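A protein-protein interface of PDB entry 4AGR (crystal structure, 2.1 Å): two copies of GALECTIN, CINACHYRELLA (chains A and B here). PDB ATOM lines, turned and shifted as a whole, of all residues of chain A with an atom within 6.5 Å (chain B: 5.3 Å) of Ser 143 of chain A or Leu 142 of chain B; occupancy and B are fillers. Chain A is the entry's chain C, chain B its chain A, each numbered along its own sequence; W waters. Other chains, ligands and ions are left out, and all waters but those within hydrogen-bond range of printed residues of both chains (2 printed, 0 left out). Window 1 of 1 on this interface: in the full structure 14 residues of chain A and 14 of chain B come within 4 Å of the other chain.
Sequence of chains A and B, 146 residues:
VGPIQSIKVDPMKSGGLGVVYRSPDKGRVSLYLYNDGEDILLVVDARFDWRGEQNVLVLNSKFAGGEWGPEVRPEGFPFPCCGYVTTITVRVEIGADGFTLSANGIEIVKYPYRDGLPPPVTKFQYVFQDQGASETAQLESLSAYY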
ATOM      1  N   ILE A   7     -12.874 -26.345   9.702  1.00  0.00           N
ATOM      2  CA  ILE A   7     -13.866 -25.282   9.576  1.00  0.00           C
ATOM      3  C   ILE A   7     -13.115 -24.011   9.794  1.00  0.00           C
ATOM      4  O   ILE A   7     -12.263 -23.933  10.674  1.00  0.00           O
ATOM      5  CB  ILE A   7     -15.052 -25.345  10.599  1.00  0.00           C
ATOM      6  CG1 ILE A   7     -14.546 -25.394  12.044  1.00  0.00           C
ATOM      7  CG2 ILE A   7     -15.991 -26.520  10.291  1.00  0.00           C
ATOM      8  CD1 ILE A   7     -15.661 -25.484  13.094  1.00  0.00           C
ATOM      9  N   GLY A  16     -15.532 -21.236  21.925  1.00  0.00           N
ATOM     10  CA  GLY A  16     -14.868 -22.522  21.976  1.00  0.00           C
ATOM     11  C   GLY A  16     -14.897 -23.148  20.592  1.00  0.00           C
ATOM     12  O   GLY A  16     -15.712 -22.742  19.731  1.00  0.00           O
ATOM     13  N   LEU A  17     -14.007 -24.141  20.394  1.00  0.00           N
ATOM     14  CA  LEU A  17     -14.031 -25.047  19.262  1.00  0.00           C
ATOM     15  C   LEU A  17     -14.201 -26.473  19.847  1.00  0.00           C
ATOM     16  O   LEU A  17     -13.548 -26.823  20.808  1.00  0.00           O
ATOM     17  CB  LEU A  17     -12.729 -24.925  18.493  1.00  0.00           C
ATOM     18  CG  LEU A  17     -12.574 -23.509  17.911  1.00  0.00           C
ATOM     19  CD1 LEU A  17     -11.111 -23.299  17.539  1.00  0.00           C
ATOM     20  CD2 LEU A  17     -13.532 -23.273  16.751  1.00  0.00           C
ATOM     21  N   GLY A  18     -15.117 -27.242  19.297  1.00  0.00           N
ATOM     22  CA  GLY A  18     -15.282 -28.611  19.699  1.00  0.00           C
ATOM     23  C   GLY A  18     -15.154 -29.621  18.533  1.00  0.00           C
ATOM     24  O   GLY A  18     -15.322 -29.259  17.366  1.00  0.00           O
ATOM     25  N   VAL A  19     -14.889 -30.886  18.878  1.00  0.00           N
ATOM     26  CA  VAL A  19     -14.859 -31.994  17.928  1.00  0.00           C
ATOM     27  C   VAL A  19     -15.443 -33.230  18.646  1.00  0.00           C
ATOM     28  O   VAL A  19     -15.217 -33.447  19.854  1.00  0.00           O
ATOM     29  CB  VAL A  19     -13.417 -32.309  17.458  1.00  0.00           C
ATOM     30  CG1 VAL A  19     -12.533 -32.638  18.668  1.00  0.00           C
ATOM     31  CG2 VAL A  19     -13.374 -33.432  16.424  1.00  0.00           C
ATOM     32  N   VAL A  20     -16.190 -34.049  17.905  1.00  0.00           N
ATOM     33  CA  VAL A  20     -16.539 -35.377  18.402  1.00  0.00           C
ATOM     34  C   VAL A  20     -15.966 -36.358  17.364  1.00  0.00           C
ATOM     35  O   VAL A  20     -16.099 -36.164  16.128  1.00  0.00           O
ATOM     36  CB  VAL A  20     -18.080 -35.572  18.541  1.00  0.00           C
ATOM     37  CG1 VAL A  20     -18.405 -37.012  19.011  1.00  0.00           C
ATOM     38  CG2 VAL A  20     -18.727 -34.463  19.451  1.00  0.00           C
ATOM     39  N   PHE A 124      -9.847 -24.257  12.371  1.00  0.00           N
ATOM     40  CA  PHE A 124      -9.852 -25.390  13.284  1.00  0.00           C
ATOM     41  C   PHE A 124      -9.883 -26.669  12.471  1.00  0.00           C
ATOM     42  O   PHE A 124     -10.868 -26.935  11.796  1.00  0.00           O
ATOM     43  CB  PHE A 124     -11.149 -25.356  14.174  1.00  0.00           C
ATOM     44  CG  PHE A 124     -11.184 -26.413  15.267  1.00  0.00           C
ATOM     45  CD1 PHE A 124     -10.095 -26.585  16.148  1.00  0.00           C
ATOM     46  CD2 PHE A 124     -12.305 -27.187  15.461  1.00  0.00           C
ATOM     47  CE1 PHE A 124     -10.136 -27.522  17.158  1.00  0.00           C
ATOM     48  CE2 PHE A 124     -12.352 -28.153  16.483  1.00  0.00           C
ATOM     49  CZ  PHE A 124     -11.263 -28.330  17.314  1.00  0.00           C
ATOM     50  N   SER A 141     -18.173 -34.750  14.188  1.00  0.00           N
ATOM     51  CA  SER A 141     -18.510 -33.343  14.036  1.00  0.00           C
ATOM     52  C   SER A 141     -17.421 -32.362  14.384  1.00  0.00           C
ATOM     53  O   SER A 141     -16.511 -32.675  15.181  1.00  0.00           O
ATOM     54  CB  SER A 141     -19.783 -33.007  14.847  1.00  0.00           C
ATOM     55  OG  SER A 141     -19.574 -33.176  16.242  1.00  0.00           O
ATOM     56  N   LEU A 142     -17.556 -31.153  13.805  1.00  0.00           N
ATOM     57  CA  LEU A 142     -16.736 -30.024  14.155  1.00  0.00           C
ATOM     58  C   LEU A 142     -17.654 -28.894  14.491  1.00  0.00           C
ATOM     59  O   LEU A 142     -18.613 -28.657  13.791  1.00  0.00           O
ATOM     60  CB  LEU A 142     -15.776 -29.646  13.016  1.00  0.00           C
ATOM     61  CG  LEU A 142     -14.520 -30.494  12.812  1.00  0.00           C
ATOM     62  CD1 LEU A 142     -13.727 -29.988  11.608  1.00  0.00           C
ATOM     63  CD2 LEU A 142     -13.570 -30.687  14.021  1.00  0.00           C
ATOM     64  N   SER A 143     -17.395 -28.214  15.596  1.00  0.00           N
ATOM     65  CA  SER A 143     -18.252 -27.120  16.023  1.00  0.00           C
ATOM     66  C   SER A 143     -17.516 -25.881  16.489  1.00  0.00           C
ATOM     67  O   SER A 143     -16.408 -25.983  17.006  1.00  0.00           O
ATOM     68  CB  SER A 143     -19.141 -27.572  17.179  1.00  0.00           C
ATOM     69  OG  SER A 143     -19.896 -28.683  16.791  1.00  0.00           O
ATOM     70  N   ALA A 144     -18.176 -24.713  16.323  1.00  0.00           N
ATOM     71  CA  ALA A 144     -17.721 -23.452  16.934  1.00  0.00           C
ATOM     72  C   ALA A 144     -18.740 -23.033  17.992  1.00  0.00           C
ATOM     73  O   ALA A 144     -19.928 -23.066  17.749  1.00  0.00           O
ATOM     74  CB  ALA A 144     -17.598 -22.362  15.859  1.00  0.00           C
ATOM     75  N   TYR A 145     -18.271 -22.615  19.160  1.00  0.00           N
ATOM     76  CA  TYR A 145     -19.194 -22.174  20.218  1.00  0.00           C
ATOM     77  C   TYR A 145     -18.958 -20.695  20.450  1.00  0.00           C
ATOM     78  O   TYR A 145     -17.815 -20.247  20.616  1.00  0.00           O
ATOM     79  CB  TYR A 145     -18.988 -22.987  21.532  1.00  0.00           C
ATOM     80  CG  TYR A 145     -19.319 -24.459  21.331  1.00  0.00           C
ATOM     81  CD1 TYR A 145     -20.617 -24.918  21.447  1.00  0.00           C
ATOM     82  CD2 TYR A 145     -18.331 -25.371  20.994  1.00  0.00           C
ATOM     83  CE1 TYR A 145     -20.939 -26.269  21.219  1.00  0.00           C
ATOM     84  CE2 TYR A 145     -18.633 -26.713  20.764  1.00  0.00           C
ATOM     85  CZ  TYR A 145     -19.930 -27.161  20.874  1.00  0.00           C
ATOM     86  OH  TYR A 145     -20.207 -28.504  20.629  1.00  0.00           O
ATOM     87  N   TYR A 146     -20.036 -19.940  20.450  1.00  0.00           N
ATOM     88  CA  TYR A 146     -19.926 -18.492  20.499  1.00  0.00           C
ATOM     89  C   TYR A 146     -20.255 -18.012  21.888  1.00  0.00           C
ATOM     90  O   TYR A 146     -19.752 -16.951  22.265  1.00  0.00           O
ATOM     91  CB  TYR A 146     -20.874 -17.863  19.450  1.00  0.00           C
ATOM     92  CG  TYR A 146     -20.383 -18.255  18.078  1.00  0.00           C
ATOM     93  CD1 TYR A 146     -19.337 -17.541  17.463  1.00  0.00           C
ATOM     94  CD2 TYR A 146     -20.863 -19.409  17.462  1.00  0.00           C
ATOM     95  CE1 TYR A 146     -18.838 -17.930  16.237  1.00  0.00           C
ATOM     96  CE2 TYR A 146     -20.394 -19.789  16.216  1.00  0.00           C
ATOM     97  CZ  TYR A 146     -19.372 -19.045  15.609  1.00  0.00           C
ATOM     98  OH  TYR A 146     -18.883 -19.456  14.375  1.00  0.00           O
ATOM     99  OXT TYR A 146     -20.993 -18.688  22.638  1.00  0.00           O
ATOM    100  N   GLN B   5     -22.429 -14.839  11.687  1.00  0.00           N
ATOM    101  CA  GLN B   5     -21.299 -15.771  11.807  1.00  0.00           C
ATOM    102  C   GLN B   5     -21.358 -16.864  10.784  1.00  0.00           C
ATOM    103  O   GLN B   5     -22.408 -17.281  10.341  1.00  0.00           O
ATOM    104  CB  GLN B   5     -21.206 -16.427  13.186  1.00  0.00           C
ATOM    105  CG  GLN B   5     -21.047 -15.490  14.351  1.00  0.00           C
ATOM    106  CD  GLN B   5     -19.692 -14.853  14.427  1.00  0.00           C
ATOM    107  OE1 GLN B   5     -18.640 -15.454  14.115  1.00  0.00           O
ATOM    108  NE2 GLN B   5     -19.697 -13.617  14.856  1.00  0.00           N
ATOM    109  N   SER B   6     -20.199 -17.331  10.410  1.00  0.00           N
ATOM    110  CA  SER B   6     -20.102 -18.351   9.404  1.00  0.00           C
ATOM    111  C   SER B   6     -19.035 -19.274   9.799  1.00  0.00           C
ATOM    112  O   SER B   6     -18.068 -18.894  10.480  1.00  0.00           O
ATOM    113  CB  SER B   6     -19.680 -17.766   8.061  1.00  0.00           C
ATOM    114  OG  SER B   6     -20.672 -16.883   7.658  1.00  0.00           O
ATOM    115  N   ILE B   7     -19.215 -20.482   9.307  1.00  0.00           N
ATOM    116  CA  ILE B   7     -18.179 -21.495   9.245  1.00  0.00           C
ATOM    117  C   ILE B   7     -18.030 -21.850   7.777  1.00  0.00           C
ATOM    118  O   ILE B   7     -18.999 -22.015   7.067  1.00  0.00           O
ATOM    119  CB  ILE B   7     -18.524 -22.779  10.114  1.00  0.00           C
ATOM    120  CG1 ILE B   7     -19.903 -23.361   9.760  1.00  0.00           C
ATOM    121  CG2 ILE B   7     -18.582 -22.423  11.607  1.00  0.00           C
ATOM    122  CD1 ILE B   7     -20.165 -24.734  10.437  1.00  0.00           C
ATOM    123  N   GLY B  18     -25.551 -27.806  11.428  1.00  0.00           N
ATOM    124  CA  GLY B  18     -26.458 -27.483  12.513  1.00  0.00           C
ATOM    125  C   GLY B  18     -26.178 -26.113  13.142  1.00  0.00           C
ATOM    126  O   GLY B  18     -25.096 -25.576  13.068  1.00  0.00           O
ATOM    127  N   VAL B  19     -27.181 -25.568  13.785  1.00  0.00           N
ATOM    128  CA  VAL B  19     -27.052 -24.276  14.436  1.00  0.00           C
ATOM    129  C   VAL B  19     -27.892 -24.434  15.668  1.00  0.00           C
ATOM    130  O   VAL B  19     -28.906 -25.107  15.643  1.00  0.00           O
ATOM    131  CB  VAL B  19     -27.577 -23.106  13.538  1.00  0.00           C
ATOM    132  CG1 VAL B  19     -29.047 -23.328  13.180  1.00  0.00           C
ATOM    133  CG2 VAL B  19     -27.398 -21.714  14.222  1.00  0.00           C
ATOM    134  N   PHE B 124     -21.843 -22.172   5.689  1.00  0.00           N
ATOM    135  CA  PHE B 124     -23.080 -22.119   6.443  1.00  0.00           C
ATOM    136  C   PHE B 124     -23.049 -20.855   7.264  1.00  0.00           C
ATOM    137  O   PHE B 124     -22.101 -20.670   8.068  1.00  0.00           O
ATOM    138  CB  PHE B 124     -23.106 -23.320   7.383  1.00  0.00           C
ATOM    139  CG  PHE B 124     -24.375 -23.480   8.167  1.00  0.00           C
ATOM    140  CD1 PHE B 124     -25.588 -23.322   7.569  1.00  0.00           C
ATOM    141  CD2 PHE B 124     -24.323 -23.867   9.516  1.00  0.00           C
ATOM    142  CE1 PHE B 124     -26.760 -23.535   8.287  1.00  0.00           C
ATOM    143  CE2 PHE B 124     -25.476 -24.067  10.252  1.00  0.00           C
ATOM    144  CZ  PHE B 124     -26.708 -23.871   9.635  1.00  0.00           C
ATOM    145  N   TYR B 126     -25.140 -17.819   9.709  1.00  0.00           N
ATOM    146  CA  TYR B 126     -26.270 -17.351  10.522  1.00  0.00           C
ATOM    147  C   TYR B 126     -26.275 -15.843  10.438  1.00  0.00           C
ATOM    148  O   TYR B 126     -25.200 -15.231  10.543  1.00  0.00           O
ATOM    149  CB  TYR B 126     -26.044 -17.763  11.982  1.00  0.00           C
ATOM    150  CG  TYR B 126     -26.804 -17.044  13.098  1.00  0.00           C
ATOM    151  CD1 TYR B 126     -26.344 -15.831  13.617  1.00  0.00           C
ATOM    152  CD2 TYR B 126     -27.899 -17.641  13.732  1.00  0.00           C
ATOM    153  CE1 TYR B 126     -27.002 -15.184  14.669  1.00  0.00           C
ATOM    154  CE2 TYR B 126     -28.569 -16.999  14.789  1.00  0.00           C
ATOM    155  CZ  TYR B 126     -28.081 -15.790  15.259  1.00  0.00           C
ATOM    156  OH  TYR B 126     -28.719 -15.141  16.287  1.00  0.00           O
ATOM    157  N   LEU B 139     -26.549 -16.252  19.145  1.00  0.00           N
ATOM    158  CA  LEU B 139     -25.992 -17.447  18.501  1.00  0.00           C
ATOM    159  C   LEU B 139     -25.267 -18.306  19.530  1.00  0.00           C
ATOM    160  O   LEU B 139     -24.440 -17.829  20.265  1.00  0.00           O
ATOM    161  CB  LEU B 139     -25.039 -17.056  17.386  1.00  0.00           C
ATOM    162  CG  LEU B 139     -24.316 -18.162  16.628  1.00  0.00           C
ATOM    163  CD1 LEU B 139     -25.267 -19.170  15.988  1.00  0.00           C
ATOM    164  CD2 LEU B 139     -23.318 -17.685  15.584  1.00  0.00           C
ATOM    165  N   GLU B 140     -25.502 -19.597  19.570  1.00  0.00           N
ATOM    166  CA  GLU B 140     -24.735 -20.378  20.561  1.00  0.00           C
ATOM    167  C   GLU B 140     -23.658 -21.267  19.969  1.00  0.00           C
ATOM    168  O   GLU B 140     -22.641 -21.486  20.604  1.00  0.00           O
ATOM    169  CB  GLU B 140     -25.681 -21.139  21.519  1.00  0.00           C
ATOM    170  CG  GLU B 140     -26.422 -20.152  22.426  1.00  0.00           C
ATOM    171  CD  GLU B 140     -27.638 -20.754  23.147  1.00  0.00           C
ATOM    172  OE1 GLU B 140     -27.852 -21.985  23.079  1.00  0.00           O
ATOM    173  OE2 GLU B 140     -28.382 -20.010  23.811  1.00  0.00           O
ATOM    174  N   SER B 141     -23.904 -21.837  18.803  1.00  0.00           N
ATOM    175  CA  SER B 141     -22.914 -22.688  18.143  1.00  0.00           C
ATOM    176  C   SER B 141     -23.216 -22.928  16.685  1.00  0.00           C
ATOM    177  O   SER B 141     -24.346 -22.930  16.300  1.00  0.00           O
ATOM    178  CB  SER B 141     -22.880 -24.049  18.825  1.00  0.00           C
ATOM    179  OG  SER B 141     -24.103 -24.728  18.616  1.00  0.00           O
ATOM    180  N   LEU B 142     -22.206 -23.251  15.892  1.00  0.00           N
ATOM    181  CA  LEU B 142     -22.478 -23.657  14.506  1.00  0.00           C
ATOM    182  C   LEU B 142     -21.660 -24.914  14.324  1.00  0.00           C
ATOM    183  O   LEU B 142     -20.496 -24.940  14.769  1.00  0.00           O
ATOM    184  CB  LEU B 142     -21.994 -22.604  13.507  1.00  0.00           C
ATOM    185  CG  LEU B 142     -22.743 -21.285  13.400  1.00  0.00           C
ATOM    186  CD1 LEU B 142     -21.900 -20.257  12.655  1.00  0.00           C
ATOM    187  CD2 LEU B 142     -24.127 -21.405  12.730  1.00  0.00           C
ATOM    188  N   SER B 143     -22.243 -25.910  13.642  1.00  0.00           N
ATOM    189  CA  SER B 143     -21.691 -27.273  13.571  1.00  0.00           C
ATOM    190  C   SER B 143     -21.616 -27.843  12.158  1.00  0.00           C
ATOM    191  O   SER B 143     -22.506 -27.651  11.358  1.00  0.00           O
ATOM    192  CB  SER B 143     -22.606 -28.224  14.381  1.00  0.00           C
ATOM    193  OG  SER B 143     -22.341 -28.073  15.743  1.00  0.00           O
ATOM    194  N   ALA B 144     -20.604 -28.648  11.904  1.00  0.00           N
ATOM    195  CA  ALA B 144     -20.620 -29.467  10.718  1.00  0.00           C
ATOM    196  C   ALA B 144     -20.609 -30.936  11.152  1.00  0.00           C
ATOM    197  O   ALA B 144     -19.783 -31.331  11.994  1.00  0.00           O
ATOM    198  CB  ALA B 144     -19.404 -29.144   9.861  1.00  0.00           C
HETATM  199  O   HOH W   1     -21.948 -21.096  23.066  1.00  0.00           O
HETATM  200  O   HOH W   2     -17.552 -17.616  12.726  1.00  0.00           O
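O of Glu 140 of chain B is in hydrogen-bond range of N of Tyr 146 of chain A (3.0 Å).
The side-chain hydroxyl (OG) of Ser 143 of chain A sits at hydrogen-bond distance from the side-chain hydroxyl (OG) of Ser 143 of chain B.
The backbone NH of Ala 144 of chain B is in hydrogen-bond range of the backbone carbonyl oxygen of Leu 142 of chain A.
O of Leu 142 of chain B sits at hydrogen-bond distance from N of Ala 144 of chain A (2.8 Å).
The backbone carbonyl oxygen of Ser 141 of chain A lies within hydrogen-bond range of the backbone NH of Val 20 of chain A, at 3.1 Å.
O of Gln 5 of chain B lies within hydrogen-bond range of N of Tyr 126 of chain B, 2.9 Å away.
The backbone carbonyl oxygen of Gly 18 of chain B sits at hydrogen-bond distance from the backbone NH of Ser 143 of chain B, at 2.9 Å.
N of Gly 18 of chain A lies within hydrogen-bond range of O of Ser 143 of chain A (2.9 Å).
The backbone carbonyl oxygen (O) of Gly 16 of chain A sits at hydrogen-bond distance from the backbone NH (N) of Tyr 145 of chain A (2.6 Å).
Among the printed residues, pairs that only touch across the chains: Ser 141 of chain A with Ala 144 of chain B (3.1 Å), Leu 142 of chain A with Ser 143 of chain B (3.4 Å), Ser 143 of chain A with Leu 142 of chain B (3.4 Å), Ala 144 of chain A with Ser 141 of chain B (3.0 Å), Tyr 145 of chain A with Glu 140 of chain B (3.5 Å), Tyr 145 of chain A with Ser 141 of chain B (3.6 Å), Tyr 146 of chain A with Gln 5 of chain B (3.3 Å), Tyr 146 of chain A with Leu 139 of chain B (3.5 Å), Tyr 146 of chain A with Ser 141 of chain B (3.9 Å) and Tyr 146 of chain A with Leu 142 of chain B (3.6 Å).
Ser 143 of chain A touches just these residues of chain B: Leu 142 (3.4 Å) and Ser 143 (2.7 Å).
Printed residues of chain A within 4 Å of Gln 5 of chain B: Tyr 146 (3.3 Å).
Ser 6 of chain B touches none of the printed residues of chain A.
Of the printed residues of chain A, Leu 139 of chain B touches Tyr 146 (3.5 Å).
Of chain A, only Ser 143 (3.4 Å), Ala 144 (2.8 Å) and Tyr 146 (3.6 Å) come within 4 Å of Leu 142 of chain B.
The nearest residue of chain B that does not touch Ser 143 of chain A is Ala 144 of chain B (4.9 Å).
The nearest printed residue of chain B that does not touch Ser 141 of chain A is Ser 143 of chain B (5.6 Å).
Printed residues of chain B that touch a printed residue of chain A: Gln 5, Leu 139, Glu 140, Ser 141, Leu 142, Ser 143 and Ala 144.
Hydrophobic or aromatic side chains of chain B that line the printed part of chain A: Leu 139 and Leu 142.
Among the printed residues, 14 pairs touch across the chains.
Among the printed residues, no Asp or Glu carboxylate lies within 4 Å of a Lys or Arg side-chain nitrogen of the other chain.
Ser 141 of chain A touches Ala 144 of chain B, and with the chains exchanged Ala 144 of chain A touches Ser 141 of chain B.
Leu 142 of chain A touches Ser 143 of chain B, and with the chains exchanged Ser 143 of chain A touches Leu 142 of chain B.
Leu 142 of chain A touches Ala 144 of chain B, and with the chains exchanged Ala 144 of chain A touches Leu 142 of chain B.
Ser 143 of chain A touches its own counterpart, Ser 143 of chain B.
Water W1 bridges the backbone carbonyl oxygen (O) of Glu 140 of chain B (2.6 Å) and the chain-end carboxylate (OXT) of Tyr 146 of chain A (2.6 Å).
Water W2 lies within hydrogen-bond range of O of Ser 6 of chain B (2.6 Å), OE1 of Gln 5 of chain B (2.8 Å) and OH of Tyr 146 of chain A (2.8 Å).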
